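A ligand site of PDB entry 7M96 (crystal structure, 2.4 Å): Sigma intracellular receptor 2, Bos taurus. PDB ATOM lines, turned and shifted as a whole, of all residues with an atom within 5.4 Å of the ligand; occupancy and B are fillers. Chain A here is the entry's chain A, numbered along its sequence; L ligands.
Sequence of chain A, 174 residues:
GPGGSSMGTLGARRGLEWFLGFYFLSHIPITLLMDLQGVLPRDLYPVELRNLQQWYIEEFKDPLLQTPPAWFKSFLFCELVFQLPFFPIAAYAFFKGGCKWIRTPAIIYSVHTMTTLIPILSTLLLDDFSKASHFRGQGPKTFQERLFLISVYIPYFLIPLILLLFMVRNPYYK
An oxygen (O2) of the ligand lies within hydrogen-bond range of the side-chain amide nitrogen (NE2) of Gln 83 (2.4 Å). The side-chain carboxylate of Asp 35 is in salt-bridge range of a nitrogen (N2) of the ligand, 2.8 Å away. O of Val 152 sits at hydrogen-bond distance from O1 of the ligand (2.9 Å).
NE2 of Gln 83 sits at hydrogen-bond distance from NE2 of His 112 (3.1 Å). The backbone NH of Asp 35 is in hydrogen-bond range of the backbone carbonyl oxygen of Ile 30, 3.1 Å away. OH of Tyr 153 is in hydrogen-bond range of OD2 of Asp 62, 2.6 Å away. The side-chain carboxylate of Asp 62 is in hydrogen-bond range of the side-chain hydroxyl of Tyr 56, at 2.7 Å. The side-chain carboxylate of Asp 62 is in hydrogen-bond range of the backbone NH of Leu 65 (3.2 Å).
Merely in contact with the ligand: Tyr 156 (3.0 Å), Tyr 153 (3.5 Å), Thr 116 (3.5 Å), Phe 75 (3.5 Å), Glu 79 (3.5 Å), Ile 30 (3.6 Å), Tyr 56 (3.7 Å), Leu 65 (3.7 Å), Thr 113 (3.8 Å), His 27 (3.8 Å) and Met 34 (3.9 Å). Hydrophobic or aromatic side chains that line the ligand: His 27, Ile 30, Met 34, Leu 65, Phe 75, Val 152, Tyr 153 and Tyr 156. Of the 20 residues printed, 14 come within 4 Å of the ligand. Along chain A the residues within 4 Å of the ligand span positions 27 to 156.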
ATOM      1  N   HIS A  27      -4.135  37.053   4.034  1.00  0.00           N
ATOM      2  CA  HIS A  27      -3.317  35.845   4.064  1.00  0.00           C
ATOM      3  C   HIS A  27      -2.476  35.697   2.801  1.00  0.00           C
ATOM      4  O   HIS A  27      -1.475  34.962   2.829  1.00  0.00           O
ATOM      5  CB  HIS A  27      -4.215  34.624   4.261  1.00  0.00           C
ATOM      6  CG  HIS A  27      -3.547  33.472   4.946  1.00  0.00           C
ATOM      7  ND1 HIS A  27      -2.183  33.285   4.938  1.00  0.00           N
ATOM      8  CD2 HIS A  27      -4.061  32.449   5.680  1.00  0.00           C
ATOM      9  CE1 HIS A  27      -1.877  32.191   5.628  1.00  0.00           C
ATOM     10  NE2 HIS A  27      -3.003  31.675   6.088  1.00  0.00           N
ATOM     11  N   ILE A  30       0.875  37.741   3.338  1.00  0.00           N
ATOM     12  CA  ILE A  30       1.617  37.087   4.412  1.00  0.00           C
ATOM     13  C   ILE A  30       2.263  35.797   3.922  1.00  0.00           C
ATOM     14  O   ILE A  30       3.433  35.523   4.207  1.00  0.00           O
ATOM     15  CB  ILE A  30       0.689  36.835   5.617  1.00  0.00           C
ATOM     16  CG1 ILE A  30       0.231  38.162   6.215  1.00  0.00           C
ATOM     17  CG2 ILE A  30       1.374  35.961   6.659  1.00  0.00           C
ATOM     18  CD1 ILE A  30      -0.783  38.022   7.322  1.00  0.00           C
ATOM     19  N   MET A  34       6.391  36.276   3.231  1.00  0.00           N
ATOM     20  CA  MET A  34       7.012  35.910   4.489  1.00  0.00           C
ATOM     21  C   MET A  34       7.092  34.398   4.678  1.00  0.00           C
ATOM     22  O   MET A  34       8.177  33.849   4.940  1.00  0.00           O
ATOM     23  CB  MET A  34       6.255  36.544   5.661  1.00  0.00           C
ATOM     24  CG  MET A  34       6.958  36.429   6.995  1.00  0.00           C
ATOM     25  SD  MET A  34       8.475  37.406   7.076  1.00  0.00           S
ATOM     26  CE  MET A  34       7.827  39.047   6.745  1.00  0.00           C
ATOM     27  N   ASP A  35       5.954  33.712   4.552  1.00  0.00           N
ATOM     28  CA  ASP A  35       5.909  32.279   4.858  1.00  0.00           C
ATOM     29  C   ASP A  35       6.725  31.463   3.867  1.00  0.00           C
ATOM     30  O   ASP A  35       7.451  30.538   4.259  1.00  0.00           O
ATOM     31  CB  ASP A  35       4.465  31.791   4.893  1.00  0.00           C
ATOM     32  CG  ASP A  35       3.785  32.057   6.222  1.00  0.00           C
ATOM     33  OD1 ASP A  35       4.463  31.945   7.264  1.00  0.00           O
ATOM     34  OD2 ASP A  35       2.581  32.375   6.223  1.00  0.00           O
ATOM     35  N   TYR A  56      12.456  39.168  11.756  1.00  0.00           N
ATOM     36  CA  TYR A  56      11.485  38.376  12.488  1.00  0.00           C
ATOM     37  C   TYR A  56      12.118  37.130  13.100  1.00  0.00           C
ATOM     38  O   TYR A  56      11.779  36.742  14.221  1.00  0.00           O
ATOM     39  CB  TYR A  56      10.321  37.996  11.572  1.00  0.00           C
ATOM     40  CG  TYR A  56       9.452  36.888  12.120  1.00  0.00           C
ATOM     41  CD1 TYR A  56       8.480  37.152  13.068  1.00  0.00           C
ATOM     42  CD2 TYR A  56       9.599  35.576  11.676  1.00  0.00           C
ATOM     43  CE1 TYR A  56       7.679  36.143  13.578  1.00  0.00           C
ATOM     44  CE2 TYR A  56       8.800  34.565  12.172  1.00  0.00           C
ATOM     45  CZ  TYR A  56       7.845  34.857  13.119  1.00  0.00           C
ATOM     46  OH  TYR A  56       7.060  33.845  13.617  1.00  0.00           O
ATOM     47  N   ASP A  62      12.305  32.430  15.818  1.00  0.00           N
ATOM     48  CA  ASP A  62      11.516  31.433  15.090  1.00  0.00           C
ATOM     49  C   ASP A  62      12.446  30.311  14.615  1.00  0.00           C
ATOM     50  O   ASP A  62      13.382  30.578  13.862  1.00  0.00           O
ATOM     51  CB  ASP A  62      10.792  32.084  13.904  1.00  0.00           C
ATOM     52  CG  ASP A  62       9.706  31.201  13.320  1.00  0.00           C
ATOM     53  OD1 ASP A  62       9.983  30.017  13.001  1.00  0.00           O
ATOM     54  OD2 ASP A  62       8.559  31.678  13.166  1.00  0.00           O
ATOM     55  N   LEU A  65      11.052  28.671  10.328  1.00  0.00           N
ATOM     56  CA  LEU A  65      10.917  29.335   9.032  1.00  0.00           C
ATOM     57  C   LEU A  65      12.233  29.451   8.275  1.00  0.00           C
ATOM     58  O   LEU A  65      12.255  29.301   7.044  1.00  0.00           O
ATOM     59  CB  LEU A  65      10.310  30.730   9.219  1.00  0.00           C
ATOM     60  CG  LEU A  65       8.824  30.845   8.857  1.00  0.00           C
ATOM     61  CD1 LEU A  65       8.353  32.288   8.994  1.00  0.00           C
ATOM     62  CD2 LEU A  65       8.571  30.318   7.459  1.00  0.00           C
ATOM     63  N   PHE A  72       7.830  20.413   8.381  1.00  0.00           N
ATOM     64  CA  PHE A  72       7.374  21.791   8.196  1.00  0.00           C
ATOM     65  C   PHE A  72       7.505  22.223   6.744  1.00  0.00           C
ATOM     66  O   PHE A  72       6.745  23.085   6.290  1.00  0.00           O
ATOM     67  CB  PHE A  72       8.168  22.726   9.119  1.00  0.00           C
ATOM     68  CG  PHE A  72       7.636  24.126   9.151  1.00  0.00           C
ATOM     69  CD1 PHE A  72       6.601  24.470  10.009  1.00  0.00           C
ATOM     70  CD2 PHE A  72       8.193  25.107   8.350  1.00  0.00           C
ATOM     71  CE1 PHE A  72       6.120  25.764  10.054  1.00  0.00           C
ATOM     72  CE2 PHE A  72       7.713  26.410   8.394  1.00  0.00           C
ATOM     73  CZ  PHE A  72       6.677  26.733   9.239  1.00  0.00           C
ATOM     74  N   PHE A  75       4.365  21.247   4.740  1.00  0.00           N
ATOM     75  CA  PHE A  75       3.207  22.104   5.013  1.00  0.00           C
ATOM     76  C   PHE A  75       3.286  23.401   4.226  1.00  0.00           C
ATOM     77  O   PHE A  75       2.257  23.923   3.774  1.00  0.00           O
ATOM     78  CB  PHE A  75       3.107  22.383   6.512  1.00  0.00           C
ATOM     79  CG  PHE A  75       2.580  21.227   7.318  1.00  0.00           C
ATOM     80  CD1 PHE A  75       1.667  20.335   6.767  1.00  0.00           C
ATOM     81  CD2 PHE A  75       2.996  21.024   8.627  1.00  0.00           C
ATOM     82  CE1 PHE A  75       1.176  19.269   7.509  1.00  0.00           C
ATOM     83  CE2 PHE A  75       2.506  19.968   9.368  1.00  0.00           C
ATOM     84  CZ  PHE A  75       1.602  19.085   8.811  1.00  0.00           C
ATOM     85  N   LEU A  76       4.491  23.947   4.055  1.00  0.00           N
ATOM     86  CA  LEU A  76       4.647  25.174   3.273  1.00  0.00           C
ATOM     87  C   LEU A  76       4.237  24.955   1.814  1.00  0.00           C
ATOM     88  O   LEU A  76       3.667  25.845   1.183  1.00  0.00           O
ATOM     89  CB  LEU A  76       6.081  25.676   3.357  1.00  0.00           C
ATOM     90  CG  LEU A  76       6.505  26.209   4.729  1.00  0.00           C
ATOM     91  CD1 LEU A  76       8.009  26.445   4.776  1.00  0.00           C
ATOM     92  CD2 LEU A  76       5.751  27.494   5.037  1.00  0.00           C
ATOM     93  N   GLU A  79       0.612  24.998   1.710  1.00  0.00           N
ATOM     94  CA  GLU A  79       0.153  26.382   1.776  1.00  0.00           C
ATOM     95  C   GLU A  79       0.260  27.059   0.413  1.00  0.00           C
ATOM     96  O   GLU A  79      -0.562  27.921   0.079  1.00  0.00           O
ATOM     97  CB  GLU A  79       0.955  27.137   2.831  1.00  0.00           C
ATOM     98  CG  GLU A  79       0.471  28.546   3.113  1.00  0.00           C
ATOM     99  CD  GLU A  79       1.376  29.270   4.093  1.00  0.00           C
ATOM    100  OE1 GLU A  79       2.406  28.692   4.494  1.00  0.00           O
ATOM    101  OE2 GLU A  79       1.057  30.425   4.467  1.00  0.00           O
ATOM    102  N   GLN A  83      -3.615  26.168  -0.406  1.00  0.00           N
ATOM    103  CA  GLN A  83      -4.228  27.249   0.359  1.00  0.00           C
ATOM    104  C   GLN A  83      -4.233  28.567  -0.429  1.00  0.00           C
ATOM    105  O   GLN A  83      -5.258  29.253  -0.476  1.00  0.00           O
ATOM    106  CB  GLN A  83      -3.491  27.433   1.690  1.00  0.00           C
ATOM    107  CG  GLN A  83      -3.538  26.205   2.603  1.00  0.00           C
ATOM    108  CD  GLN A  83      -2.680  26.374   3.845  1.00  0.00           C
ATOM    109  OE1 GLN A  83      -2.592  27.456   4.417  1.00  0.00           O
ATOM    110  NE2 GLN A  83      -2.043  25.281   4.266  1.00  0.00           N
ATOM    111  N   HIS A 112      -7.748  21.194   7.399  1.00  0.00           N
ATOM    112  CA  HIS A 112      -6.369  21.129   6.933  1.00  0.00           C
ATOM    113  C   HIS A 112      -5.496  22.154   7.648  1.00  0.00           C
ATOM    114  O   HIS A 112      -4.331  21.874   7.961  1.00  0.00           O
ATOM    115  CB  HIS A 112      -6.326  21.343   5.423  1.00  0.00           C
ATOM    116  CG  HIS A 112      -4.956  21.595   4.873  1.00  0.00           C
ATOM    117  ND1 HIS A 112      -3.980  20.625   4.846  1.00  0.00           N
ATOM    118  CD2 HIS A 112      -4.394  22.706   4.352  1.00  0.00           C
ATOM    119  CE1 HIS A 112      -2.881  21.128   4.320  1.00  0.00           C
ATOM    120  NE2 HIS A 112      -3.105  22.391   4.003  1.00  0.00           N
ATOM    121  N   THR A 113      -6.050  23.330   7.934  1.00  0.00           N
ATOM    122  CA  THR A 113      -5.272  24.381   8.582  1.00  0.00           C
ATOM    123  C   THR A 113      -5.115  24.119  10.070  1.00  0.00           C
ATOM    124  O   THR A 113      -4.064  24.417  10.648  1.00  0.00           O
ATOM    125  CB  THR A 113      -5.923  25.738   8.343  1.00  0.00           C
ATOM    126  OG1 THR A 113      -6.225  25.876   6.950  1.00  0.00           O
ATOM    127  CG2 THR A 113      -4.977  26.854   8.755  1.00  0.00           C
ATOM    128  N   THR A 116      -2.380  21.276  10.515  1.00  0.00           N
ATOM    129  CA  THR A 116      -0.971  21.617  10.284  1.00  0.00           C
ATOM    130  C   THR A 116      -0.372  22.418  11.426  1.00  0.00           C
ATOM    131  O   THR A 116       0.853  22.475  11.555  1.00  0.00           O
ATOM    132  CB  THR A 116      -0.817  22.383   8.961  1.00  0.00           C
ATOM    133  OG1 THR A 116       0.530  22.835   8.837  1.00  0.00           O
ATOM    134  CG2 THR A 116      -1.734  23.582   8.918  1.00  0.00           C
ATOM    135  N   LEU A 117      -1.204  23.029  12.280  1.00  0.00           N
ATOM    136  CA  LEU A 117      -0.707  23.857  13.361  1.00  0.00           C
ATOM    137  C   LEU A 117      -0.621  23.132  14.693  1.00  0.00           C
ATOM    138  O   LEU A 117       0.089  23.609  15.595  1.00  0.00           O
ATOM    139  CB  LEU A 117      -1.596  25.095  13.533  1.00  0.00           C
ATOM    140  CG  LEU A 117      -1.424  26.123  12.417  1.00  0.00           C
ATOM    141  CD1 LEU A 117      -2.420  27.204  12.607  1.00  0.00           C
ATOM    142  CD2 LEU A 117      -0.020  26.713  12.436  1.00  0.00           C
ATOM    143  N   ILE A 120       2.866  22.320  15.029  1.00  0.00           N
ATOM    144  CA  ILE A 120       3.662  23.542  15.105  1.00  0.00           C
ATOM    145  C   ILE A 120       3.592  24.141  16.504  1.00  0.00           C
ATOM    146  O   ILE A 120       4.620  24.427  17.124  1.00  0.00           O
ATOM    147  CB  ILE A 120       3.190  24.558  14.040  1.00  0.00           C
ATOM    148  CG1 ILE A 120       3.469  24.012  12.636  1.00  0.00           C
ATOM    149  CG2 ILE A 120       3.880  25.897  14.230  1.00  0.00           C
ATOM    150  CD1 ILE A 120       2.993  24.922  11.527  1.00  0.00           C
ATOM    151  N   VAL A 152       1.914  34.650  17.516  1.00  0.00           N
ATOM    152  CA  VAL A 152       1.826  34.970  16.089  1.00  0.00           C
ATOM    153  C   VAL A 152       1.380  33.785  15.247  1.00  0.00           C
ATOM    154  O   VAL A 152       0.958  33.976  14.104  1.00  0.00           O
ATOM    155  CB  VAL A 152       3.174  35.512  15.565  1.00  0.00           C
ATOM    156  CG1 VAL A 152       3.671  36.644  16.457  1.00  0.00           C
ATOM    157  CG2 VAL A 152       4.208  34.407  15.485  1.00  0.00           C
ATOM    158  N   TYR A 153       1.453  32.563  15.774  1.00  0.00           N
ATOM    159  CA  TYR A 153       0.993  31.374  15.067  1.00  0.00           C
ATOM    160  C   TYR A 153      -0.439  30.997  15.415  1.00  0.00           C
ATOM    161  O   TYR A 153      -1.134  30.413  14.578  1.00  0.00           O
ATOM    162  CB  TYR A 153       1.906  30.182  15.361  1.00  0.00           C
ATOM    163  CG  TYR A 153       3.181  30.154  14.536  1.00  0.00           C
ATOM    164  CD1 TYR A 153       4.273  30.931  14.882  1.00  0.00           C
ATOM    165  CD2 TYR A 153       3.292  29.316  13.431  1.00  0.00           C
ATOM    166  CE1 TYR A 153       5.440  30.895  14.136  1.00  0.00           C
ATOM    167  CE2 TYR A 153       4.454  29.281  12.677  1.00  0.00           C
ATOM    168  CZ  TYR A 153       5.523  30.072  13.039  1.00  0.00           C
ATOM    169  OH  TYR A 153       6.677  30.038  12.291  1.00  0.00           O
ATOM    170  N   TYR A 156      -3.992  31.559  13.256  1.00  0.00           N
ATOM    171  CA  TYR A 156      -4.301  30.683  12.137  1.00  0.00           C
ATOM    172  C   TYR A 156      -4.840  29.328  12.569  1.00  0.00           C
ATOM    173  O   TYR A 156      -5.093  28.481  11.707  1.00  0.00           O
ATOM    174  CB  TYR A 156      -3.056  30.513  11.261  1.00  0.00           C
ATOM    175  CG  TYR A 156      -2.553  31.831  10.720  1.00  0.00           C
ATOM    176  CD1 TYR A 156      -3.201  32.466   9.676  1.00  0.00           C
ATOM    177  CD2 TYR A 156      -1.436  32.444  11.284  1.00  0.00           C
ATOM    178  CE1 TYR A 156      -2.748  33.674   9.185  1.00  0.00           C
ATOM    179  CE2 TYR A 156      -0.970  33.641  10.796  1.00  0.00           C
ATOM    180  CZ  TYR A 156      -1.634  34.258   9.752  1.00  0.00           C
ATOM    181  OH  TYR A 156      -1.161  35.465   9.271  1.00  0.00           O
HETATM  182  C1  LIG L   1      -0.414  26.565   6.969  1.00  0.00           C
HETATM  183  C2  LIG L   1      -1.438  27.474   7.615  1.00  0.00           C
HETATM  184  C3  LIG L   1      -0.945  28.899   7.700  1.00  0.00           C
HETATM  185  C4  LIG L   1       0.457  28.957   8.258  1.00  0.00           C
HETATM  186  C5  LIG L   1       1.354  27.912   7.992  1.00  0.00           C
HETATM  187  C6  LIG L   1       2.640  27.960   8.498  1.00  0.00           C
HETATM  188  C7  LIG L   1       3.041  29.042   9.274  1.00  0.00           C
HETATM  189  N1  LIG L   1       0.910  26.824   7.210  1.00  0.00           N
HETATM  190  C8  LIG L   1       1.897  25.937   6.628  1.00  0.00           C
HETATM  191  O1  LIG L   1       1.843  34.602  11.364  1.00  0.00           O
HETATM  192  C9  LIG L   1       3.698  33.512  10.394  1.00  0.00           C
HETATM  193  C10 LIG L   1       3.934  33.156  11.861  1.00  0.00           C
HETATM  194  C11 LIG L   1       2.773  34.747  10.295  1.00  0.00           C
HETATM  195  C12 LIG L   1       3.484  36.084  10.394  1.00  0.00           C
HETATM  196  C13 LIG L   1       3.667  36.877   9.273  1.00  0.00           C
HETATM  197  C14 LIG L   1       4.288  38.103   9.365  1.00  0.00           C
HETATM  198  C15 LIG L   1       4.728  38.568  10.589  1.00  0.00           C
HETATM  199  C16 LIG L   1       4.548  37.795  11.709  1.00  0.00           C
HETATM  200  C17 LIG L   1       3.933  36.557  11.611  1.00  0.00           C
HETATM  201  C18 LIG L   1       5.062  33.777   9.762  1.00  0.00           C
HETATM  202  C19 LIG L   1       0.884  30.027   9.040  1.00  0.00           C
HETATM  203  C20 LIG L   1       2.168  30.076   9.560  1.00  0.00           C
HETATM  204  C21 LIG L   1       2.586  31.220  10.460  1.00  0.00           C
HETATM  205  N2  LIG L   1       3.042  32.389   9.693  1.00  0.00           N
HETATM  206  O2  LIG L   1      -0.753  25.635   6.269  1.00  0.00           O
